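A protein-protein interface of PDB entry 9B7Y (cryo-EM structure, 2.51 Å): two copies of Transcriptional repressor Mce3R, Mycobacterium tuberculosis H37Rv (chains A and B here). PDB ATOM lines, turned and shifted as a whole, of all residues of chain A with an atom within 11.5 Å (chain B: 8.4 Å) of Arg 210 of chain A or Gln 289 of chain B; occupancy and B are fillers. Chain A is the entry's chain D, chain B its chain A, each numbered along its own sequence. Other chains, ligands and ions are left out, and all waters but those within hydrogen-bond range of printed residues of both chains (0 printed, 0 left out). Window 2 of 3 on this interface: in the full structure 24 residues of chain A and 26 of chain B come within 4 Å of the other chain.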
ATOM      1  N   PRO A 204      15.342   8.049   7.121  1.00  0.00           N
ATOM      2  CA  PRO A 204      16.228   9.156   6.771  1.00  0.00           C
ATOM      3  C   PRO A 204      16.074  10.265   7.818  1.00  0.00           C
ATOM      4  O   PRO A 204      14.987  10.800   7.932  1.00  0.00           O
ATOM      5  CB  PRO A 204      15.681   9.630   5.420  1.00  0.00           C
ATOM      6  CG  PRO A 204      15.027   8.399   4.834  1.00  0.00           C
ATOM      7  CD  PRO A 204      14.455   7.657   6.024  1.00  0.00           C
ATOM      8  N   ALA A 205      17.151  10.581   8.542  1.00  0.00           N
ATOM      9  CA  ALA A 205      17.080  11.600   9.616  1.00  0.00           C
ATOM     10  C   ALA A 205      18.487  11.874  10.160  1.00  0.00           C
ATOM     11  O   ALA A 205      18.586  12.131  11.376  1.00  0.00           O
ATOM     12  CB  ALA A 205      16.152  11.127  10.707  1.00  0.00           C
ATOM     13  N   ALA A 208       7.966  15.512  11.175  1.00  0.00           N
ATOM     14  CA  ALA A 208       9.141  16.305  11.515  1.00  0.00           C
ATOM     15  C   ALA A 208       8.749  17.549  12.305  1.00  0.00           C
ATOM     16  O   ALA A 208       7.593  17.704  12.701  1.00  0.00           O
ATOM     17  CB  ALA A 208       9.902  16.692  10.257  1.00  0.00           C
ATOM     18  N   ALA A 209       9.724  18.433  12.534  1.00  0.00           N
ATOM     19  CA  ALA A 209       9.443  19.679  13.238  1.00  0.00           C
ATOM     20  C   ALA A 209       8.481  20.562  12.452  1.00  0.00           C
ATOM     21  O   ALA A 209       7.711  21.323  13.050  1.00  0.00           O
ATOM     22  CB  ALA A 209      10.744  20.430  13.521  1.00  0.00           C
ATOM     23  N   ARG A 210       8.516  20.480  11.120  1.00  0.00           N
ATOM     24  CA  ARG A 210       7.549  21.206  10.304  1.00  0.00           C
ATOM     25  C   ARG A 210       6.133  20.703  10.561  1.00  0.00           C
ATOM     26  O   ARG A 210       5.183  21.492  10.634  1.00  0.00           O
ATOM     27  CB  ARG A 210       7.914  21.077   8.824  1.00  0.00           C
ATOM     28  CG  ARG A 210       8.142  19.644   8.364  1.00  0.00           C
ATOM     29  CD  ARG A 210       8.047  19.515   6.855  1.00  0.00           C
ATOM     30  NE  ARG A 210       8.045  18.119   6.432  1.00  0.00           N
ATOM     31  CZ  ARG A 210       7.914  17.716   5.177  1.00  0.00           C
ATOM     32  NH1 ARG A 210       7.774  18.579   4.184  1.00  0.00           N
ATOM     33  NH2 ARG A 210       7.926  16.413   4.909  1.00  0.00           N
ATOM     34  N   ASP A 211       5.973  19.384  10.700  1.00  0.00           N
ATOM     35  CA  ASP A 211       4.654  18.822  10.969  1.00  0.00           C
ATOM     36  C   ASP A 211       4.221  19.086  12.405  1.00  0.00           C
ATOM     37  O   ASP A 211       3.026  19.035  12.719  1.00  0.00           O
ATOM     38  CB  ASP A 211       4.654  17.322  10.673  1.00  0.00           C
ATOM     39  CG  ASP A 211       4.846  17.021   9.199  1.00  0.00           C
ATOM     40  OD1 ASP A 211       4.892  17.976   8.398  1.00  0.00           O
ATOM     41  OD2 ASP A 211       4.954  15.829   8.842  1.00  0.00           O
ATOM     42  N   GLU A 212       5.177  19.359  13.295  1.00  0.00           N
ATOM     43  CA  GLU A 212       4.833  19.641  14.685  1.00  0.00           C
ATOM     44  C   GLU A 212       4.355  21.077  14.859  1.00  0.00           C
ATOM     45  O   GLU A 212       3.749  21.417  15.881  1.00  0.00           O
ATOM     46  CB  GLU A 212       6.031  19.359  15.590  1.00  0.00           C
ATOM     47  N   ALA A 213       4.623  21.936  13.875  1.00  0.00           N
ATOM     48  CA  ALA A 213       4.302  23.354  13.996  1.00  0.00           C
ATOM     49  C   ALA A 213       3.025  23.740  13.258  1.00  0.00           C
ATOM     50  O   ALA A 213       2.257  24.574  13.749  1.00  0.00           O
ATOM     51  CB  ALA A 213       5.469  24.200  13.484  1.00  0.00           C
ATOM     52  N   ASP A 214       2.782  23.156  12.082  1.00  0.00           N
ATOM     53  CA  ASP A 214       1.617  23.550  11.296  1.00  0.00           C
ATOM     54  C   ASP A 214       0.326  23.002  11.885  1.00  0.00           C
ATOM     55  O   ASP A 214      -0.743  23.592  11.688  1.00  0.00           O
ATOM     56  CB  ASP A 214       1.779  23.088   9.849  1.00  0.00           C
ATOM     57  CG  ASP A 214       2.184  21.636   9.746  1.00  0.00           C
ATOM     58  OD1 ASP A 214       2.359  20.996  10.802  1.00  0.00           O
ATOM     59  OD2 ASP A 214       2.313  21.128   8.612  1.00  0.00           O
ATOM     60  N   VAL A 215       0.397  21.879  12.606  1.00  0.00           N
ATOM     61  CA  VAL A 215      -0.799  21.313  13.215  1.00  0.00           C
ATOM     62  C   VAL A 215      -1.293  22.162  14.376  1.00  0.00           C
ATOM     63  O   VAL A 215      -2.418  21.962  14.850  1.00  0.00           O
ATOM     64  CB  VAL A 215      -0.542  19.867  13.677  1.00  0.00           C
ATOM     65  CG1 VAL A 215      -0.207  18.983  12.485  1.00  0.00           C
ATOM     66  CG2 VAL A 215       0.568  19.829  14.713  1.00  0.00           C
ATOM     67  N   LEU A 216      -0.480  23.103  14.856  1.00  0.00           N
ATOM     68  CA  LEU A 216      -0.901  24.044  15.893  1.00  0.00           C
ATOM     69  C   LEU A 216      -1.451  25.287  15.200  1.00  0.00           C
ATOM     70  O   LEU A 216      -0.807  26.336  15.113  1.00  0.00           O
ATOM     71  CB  LEU A 216       0.257  24.371  16.827  1.00  0.00           C
ATOM     72  CG  LEU A 216       1.063  23.179  17.347  1.00  0.00           C
ATOM     73  CD1 LEU A 216       2.154  23.635  18.300  1.00  0.00           C
ATOM     74  CD2 LEU A 216       0.152  22.167  18.022  1.00  0.00           C
ATOM     75  N   PHE A 217      -2.676  25.158  14.697  1.00  0.00           N
ATOM     76  CA  PHE A 217      -3.301  26.177  13.866  1.00  0.00           C
ATOM     77  C   PHE A 217      -4.133  27.171  14.665  1.00  0.00           C
ATOM     78  O   PHE A 217      -4.808  28.016  14.070  1.00  0.00           O
ATOM     79  CB  PHE A 217      -4.167  25.521  12.787  1.00  0.00           C
ATOM     80  CG  PHE A 217      -5.116  24.479  13.316  1.00  0.00           C
ATOM     81  CD1 PHE A 217      -6.325  24.842  13.885  1.00  0.00           C
ATOM     82  CD2 PHE A 217      -4.800  23.135  13.234  1.00  0.00           C
ATOM     83  CE1 PHE A 217      -7.195  23.886  14.368  1.00  0.00           C
ATOM     84  CE2 PHE A 217      -5.668  22.175  13.714  1.00  0.00           C
ATOM     85  CZ  PHE A 217      -6.866  22.550  14.281  1.00  0.00           C
ATOM     86  N   TRP A 376      11.712   7.408  21.796  1.00  0.00           N
ATOM     87  CA  TRP A 376      11.835   8.041  20.488  1.00  0.00           C
ATOM     88  C   TRP A 376      12.729   7.240  19.546  1.00  0.00           C
ATOM     89  O   TRP A 376      12.377   7.025  18.382  1.00  0.00           O
ATOM     90  CB  TRP A 376      12.366   9.467  20.642  1.00  0.00           C
ATOM     91  CG  TRP A 376      12.300  10.265  19.375  1.00  0.00           C
ATOM     92  CD1 TRP A 376      11.192  10.842  18.828  1.00  0.00           C
ATOM     93  CD2 TRP A 376      13.387  10.564  18.491  1.00  0.00           C
ATOM     94  NE1 TRP A 376      11.521  11.487  17.661  1.00  0.00           N
ATOM     95  CE2 TRP A 376      12.863  11.331  17.432  1.00  0.00           C
ATOM     96  CE3 TRP A 376      14.751  10.261  18.494  1.00  0.00           C
ATOM     97  CZ2 TRP A 376      13.655  11.798  16.386  1.00  0.00           C
ATOM     98  CZ3 TRP A 376      15.536  10.725  17.455  1.00  0.00           C
ATOM     99  CH2 TRP A 376      14.986  11.485  16.415  1.00  0.00           C
ATOM    100  N   ARG A 380      12.314   5.163  15.028  1.00  0.00           N
ATOM    101  CA  ARG A 380      12.953   5.744  13.847  1.00  0.00           C
ATOM    102  C   ARG A 380      13.345   4.653  12.850  1.00  0.00           C
ATOM    103  O   ARG A 380      14.507   4.484  12.481  1.00  0.00           O
ATOM    104  CB  ARG A 380      14.157   6.582  14.259  1.00  0.00           C
ATOM    105  CG  ARG A 380      13.920   7.429  15.496  1.00  0.00           C
ATOM    106  CD  ARG A 380      12.900   8.521  15.222  1.00  0.00           C
ATOM    107  NE  ARG A 380      13.086   9.124  13.908  1.00  0.00           N
ATOM    108  CZ  ARG A 380      12.122   9.704  13.206  1.00  0.00           C
ATOM    109  NH1 ARG A 380      10.884   9.781  13.665  1.00  0.00           N
ATOM    110  NH2 ARG A 380      12.407  10.218  12.013  1.00  0.00           N
ATOM    111  N   ALA B 284      -5.071  15.359   8.038  1.00  0.00           N
ATOM    112  CA  ALA B 284      -5.016  15.981   6.718  1.00  0.00           C
ATOM    113  C   ALA B 284      -3.895  17.010   6.637  1.00  0.00           C
ATOM    114  O   ALA B 284      -3.198  17.098   5.621  1.00  0.00           O
ATOM    115  CB  ALA B 284      -6.361  16.626   6.386  1.00  0.00           C
ATOM    116  N   LEU B 285      -3.712  17.801   7.697  1.00  0.00           N
ATOM    117  CA  LEU B 285      -2.631  18.782   7.709  1.00  0.00           C
ATOM    118  C   LEU B 285      -1.268  18.103   7.673  1.00  0.00           C
ATOM    119  O   LEU B 285      -0.349  18.577   6.995  1.00  0.00           O
ATOM    120  CB  LEU B 285      -2.750  19.683   8.939  1.00  0.00           C
ATOM    121  CG  LEU B 285      -3.798  20.798   8.883  1.00  0.00           C
ATOM    122  CD1 LEU B 285      -3.915  21.487  10.231  1.00  0.00           C
ATOM    123  CD2 LEU B 285      -3.455  21.805   7.803  1.00  0.00           C
ATOM    124  N   ARG B 286      -1.117  16.991   8.396  1.00  0.00           N
ATOM    125  CA  ARG B 286       0.173  16.310   8.441  1.00  0.00           C
ATOM    126  C   ARG B 286       0.463  15.553   7.150  1.00  0.00           C
ATOM    127  O   ARG B 286       1.631  15.348   6.804  1.00  0.00           O
ATOM    128  CB  ARG B 286       0.220  15.360   9.638  1.00  0.00           C
ATOM    129  CG  ARG B 286       1.606  14.844   9.979  1.00  0.00           C
ATOM    130  CD  ARG B 286       1.597  14.080  11.291  1.00  0.00           C
ATOM    131  NE  ARG B 286       1.398  14.957  12.438  1.00  0.00           N
ATOM    132  CZ  ARG B 286       0.601  14.682  13.460  1.00  0.00           C
ATOM    133  NH1 ARG B 286      -0.098  13.560  13.510  1.00  0.00           N
ATOM    134  NH2 ARG B 286       0.502  15.554  14.460  1.00  0.00           N
ATOM    135  N   ALA B 287      -0.578  15.131   6.427  1.00  0.00           N
ATOM    136  CA  ALA B 287      -0.365  14.305   5.242  1.00  0.00           C
ATOM    137  C   ALA B 287       0.233  15.106   4.090  1.00  0.00           C
ATOM    138  O   ALA B 287       1.159  14.635   3.419  1.00  0.00           O
ATOM    139  CB  ALA B 287      -1.680  13.654   4.814  1.00  0.00           C
ATOM    140  N   ASN B 288      -0.275  16.310   3.843  1.00  0.00           N
ATOM    141  CA  ASN B 288       0.132  17.106   2.694  1.00  0.00           C
ATOM    142  C   ASN B 288       0.676  18.457   3.139  1.00  0.00           C
ATOM    143  O   ASN B 288       0.354  18.958   4.219  1.00  0.00           O
ATOM    144  CB  ASN B 288      -1.035  17.310   1.720  1.00  0.00           C
ATOM    145  CG  ASN B 288      -1.506  16.013   1.098  1.00  0.00           C
ATOM    146  OD1 ASN B 288      -0.857  15.467   0.207  1.00  0.00           O
ATOM    147  ND2 ASN B 288      -2.640  15.510   1.568  1.00  0.00           N
ATOM    148  N   GLN B 289       1.510  19.044   2.281  1.00  0.00           N
ATOM    149  CA  GLN B 289       2.117  20.342   2.542  1.00  0.00           C
ATOM    150  C   GLN B 289       1.720  21.422   1.547  1.00  0.00           C
ATOM    151  O   GLN B 289       1.642  22.590   1.933  1.00  0.00           O
ATOM    152  CB  GLN B 289       3.649  20.224   2.557  1.00  0.00           C
ATOM    153  CG  GLN B 289       4.262  20.344   3.942  1.00  0.00           C
ATOM    154  CD  GLN B 289       3.982  19.135   4.810  1.00  0.00           C
ATOM    155  OE1 GLN B 289       4.115  17.994   4.367  1.00  0.00           O
ATOM    156  NE2 GLN B 289       3.582  19.378   6.052  1.00  0.00           N
ATOM    157  N   GLN B 290       1.472  21.074   0.287  1.00  0.00           N
ATOM    158  CA  GLN B 290       1.067  22.061  -0.699  1.00  0.00           C
ATOM    159  C   GLN B 290      -0.396  22.450  -0.501  1.00  0.00           C
ATOM    160  O   GLN B 290      -1.179  21.727   0.118  1.00  0.00           O
ATOM    161  CB  GLN B 290       1.293  21.532  -2.115  1.00  0.00           C
ATOM    162  CG  GLN B 290       2.653  20.883  -2.330  1.00  0.00           C
ATOM    163  CD  GLN B 290       3.807  21.849  -2.125  1.00  0.00           C
ATOM    164  OE1 GLN B 290       3.657  23.060  -2.289  1.00  0.00           O
ATOM    165  NE2 GLN B 290       4.967  21.314  -1.764  1.00  0.00           N
ATOM    166  N   ALA B 291      -0.758  23.613  -1.048  1.00  0.00           N
ATOM    167  CA  ALA B 291      -2.064  24.202  -0.759  1.00  0.00           C
ATOM    168  C   ALA B 291      -3.205  23.359  -1.321  1.00  0.00           C
ATOM    169  O   ALA B 291      -4.164  23.044  -0.607  1.00  0.00           O
ATOM    170  CB  ALA B 291      -2.126  25.626  -1.310  1.00  0.00           C
ATOM    171  N   ALA B 292      -3.124  22.994  -2.603  1.00  0.00           N
ATOM    172  CA  ALA B 292      -4.222  22.270  -3.237  1.00  0.00           C
ATOM    173  C   ALA B 292      -4.420  20.900  -2.601  1.00  0.00           C
ATOM    174  O   ALA B 292      -5.551  20.492  -2.307  1.00  0.00           O
ATOM    175  CB  ALA B 292      -3.965  22.138  -4.738  1.00  0.00           C
ATOM    176  N   GLN B 293      -3.330  20.174  -2.419  1.00  0.00           N
ATOM    177  CA  GLN B 293      -3.421  18.839  -1.859  1.00  0.00           C
ATOM    178  C   GLN B 293      -3.897  18.884  -0.425  1.00  0.00           C
ATOM    179  O   GLN B 293      -4.589  17.976   0.022  1.00  0.00           O
ATOM    180  CB  GLN B 293      -2.073  18.139  -1.960  1.00  0.00           C
ATOM    181  CG  GLN B 293      -1.732  17.605  -3.341  1.00  0.00           C
ATOM    182  CD  GLN B 293      -1.067  18.632  -4.235  1.00  0.00           C
ATOM    183  OE1 GLN B 293      -0.871  19.780  -3.846  1.00  0.00           O
ATOM    184  NE2 GLN B 293      -0.714  18.219  -5.444  1.00  0.00           N
ATOM    185  N   ARG B 294      -3.539  19.934   0.300  1.00  0.00           N
ATOM    186  CA  ARG B 294      -3.997  20.075   1.670  1.00  0.00           C
ATOM    187  C   ARG B 294      -5.483  20.378   1.720  1.00  0.00           C
ATOM    188  O   ARG B 294      -6.201  19.767   2.498  1.00  0.00           O
ATOM    189  CB  ARG B 294      -3.207  21.150   2.402  1.00  0.00           C
ATOM    190  CG  ARG B 294      -3.418  21.146   3.900  1.00  0.00           C
ATOM    191  CD  ARG B 294      -2.099  21.008   4.628  1.00  0.00           C
ATOM    192  NE  ARG B 294      -1.328  22.241   4.621  1.00  0.00           N
ATOM    193  CZ  ARG B 294      -0.192  22.409   5.290  1.00  0.00           C
ATOM    194  NH1 ARG B 294       0.300  21.419   6.018  1.00  0.00           N
ATOM    195  NH2 ARG B 294       0.448  23.566   5.232  1.00  0.00           N
ATOM    196  N   LEU B 295      -5.957  21.310   0.900  1.00  0.00           N
ATOM    197  CA  LEU B 295      -7.388  21.594   0.845  1.00  0.00           C
ATOM    198  C   LEU B 295      -8.177  20.348   0.464  1.00  0.00           C
ATOM    199  O   LEU B 295      -9.235  20.071   1.046  1.00  0.00           O
ATOM    200  CB  LEU B 295      -7.658  22.728  -0.142  1.00  0.00           C
ATOM    201  CG  LEU B 295      -9.046  23.367  -0.078  1.00  0.00           C
ATOM    202  CD1 LEU B 295      -9.349  23.838   1.335  1.00  0.00           C
ATOM    203  CD2 LEU B 295      -9.153  24.517  -1.064  1.00  0.00           C
ATOM    204  N   LEU B 345      -6.267  28.644   3.214  1.00  0.00           N
ATOM    205  CA  LEU B 345      -5.889  27.844   2.051  1.00  0.00           C
ATOM    206  C   LEU B 345      -6.584  28.337   0.785  1.00  0.00           C
ATOM    207  O   LEU B 345      -5.967  28.405  -0.286  1.00  0.00           O
ATOM    208  CB  LEU B 345      -6.199  26.369   2.297  1.00  0.00           C
ATOM    209  CG  LEU B 345      -5.123  25.602   3.066  1.00  0.00           C
ATOM    210  CD1 LEU B 345      -5.555  24.172   3.323  1.00  0.00           C
ATOM    211  CD2 LEU B 345      -3.807  25.638   2.308  1.00  0.00           C
ATOM    212  N   LYS B 348      -4.942  31.434  -0.413  1.00  0.00           N
ATOM    213  CA  LYS B 348      -3.677  31.094  -1.055  1.00  0.00           C
ATOM    214  C   LYS B 348      -3.897  30.585  -2.474  1.00  0.00           C
ATOM    215  O   LYS B 348      -3.163  30.960  -3.396  1.00  0.00           O
ATOM    216  CB  LYS B 348      -2.925  30.054  -0.224  1.00  0.00           C
ATOM    217  CG  LYS B 348      -1.456  30.373  -0.015  1.00  0.00           C
ATOM    218  CD  LYS B 348      -0.895  29.643   1.194  1.00  0.00           C
ATOM    219  CE  LYS B 348      -1.427  30.229   2.490  1.00  0.00           C
ATOM    220  NZ  LYS B 348      -0.530  29.932   3.642  1.00  0.00           N
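The side-chain amide nitrogen (NE2) of Gln 289 of chain B is in hydrogen-bond range of the side-chain carboxylate (OD1) of Asp 211 of chain A. NE2 of Gln 289 of chain B sits at hydrogen-bond distance from OD2 of Asp 214 of chain A, 3.4 Å away. The guanidinium group (NH1) of Arg 294 of chain B is in salt-bridge range of the side-chain carboxylate (OD2) of Asp 214 of chain A, 3.3 Å away.
The backbone carbonyl oxygen of Leu 285 of chain B lies within hydrogen-bond range of the guanidinium group of Arg 294 of chain B (3.1 Å). O of Asn 288 of chain B lies within hydrogen-bond range of NH1 of Arg 294 of chain B (3.0 Å). The guanidinium group (NE) of Arg 210 of chain A lies within salt-bridge range of the side-chain carboxylate (OD1) of Asp 211 of chain A.
Among the printed residues, pairs that only touch across the chains: Phe 217 of chain A with Leu 285 of chain B (3.5 Å), Asp 211 of chain A with Arg 286 of chain B (3.7 Å) and Arg 210 of chain A with Gln 289 of chain B (3.7 Å).
No residue of chain B comes within 4 Å of Ala 209 of chain A. Of chain B, only Gln 289 (3.7 Å) comes within 4 Å of Arg 210 of chain A. Of the printed residues of chain B, Asp 211 of chain A touches Arg 286 and Gln 289. Glu 212 of chain A touches none of the printed residues of chain B. Of the printed residues of chain B, Asp 214 of chain A touches Gln 289 and Arg 294. Of the printed residues of chain A, Arg 286 of chain B touches Asp 211 (3.7 Å). Of chain A, only Arg 210, Asp 211 and Asp 214 come within 4 Å of Gln 289 of chain B. Of the printed residues of chain A, Arg 294 of chain B touches Asp 214. The nearest printed residue of chain B that does not touch Asp 211 of chain A is Leu 285 of chain B (5.5 Å).
Of the 14 printed residues of chain B, 4 touch a printed residue of chain A. Printed residues of chain B that touch a printed residue of chain A: Leu 285, Arg 286, Gln 289 and Arg 294. Hydrophobic or aromatic side chains of chain B that line the printed part of chain A: Leu 285. Of the 14 printed residues of chain A, 4 touch a printed residue of chain B. Hydrophobic or aromatic side chains of chain A that line the printed part of chain B: Phe 217. Along chain A the printed residues that touch a printed residue of chain B span positions 210 to 217. Among the printed residues, 6 pairs touch across the chains. Among the printed residues, Asp or Glu carboxylates within 4 Å of a Lys or Arg side-chain nitrogen of the other chain: Asp 214 of chain A with Arg 294 of chain B (3.3 Å).
No position is printed for both chains. Of the 6 pairs that touch across the chains among the printed residues, none has its exchanged pair printed and touching as well.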
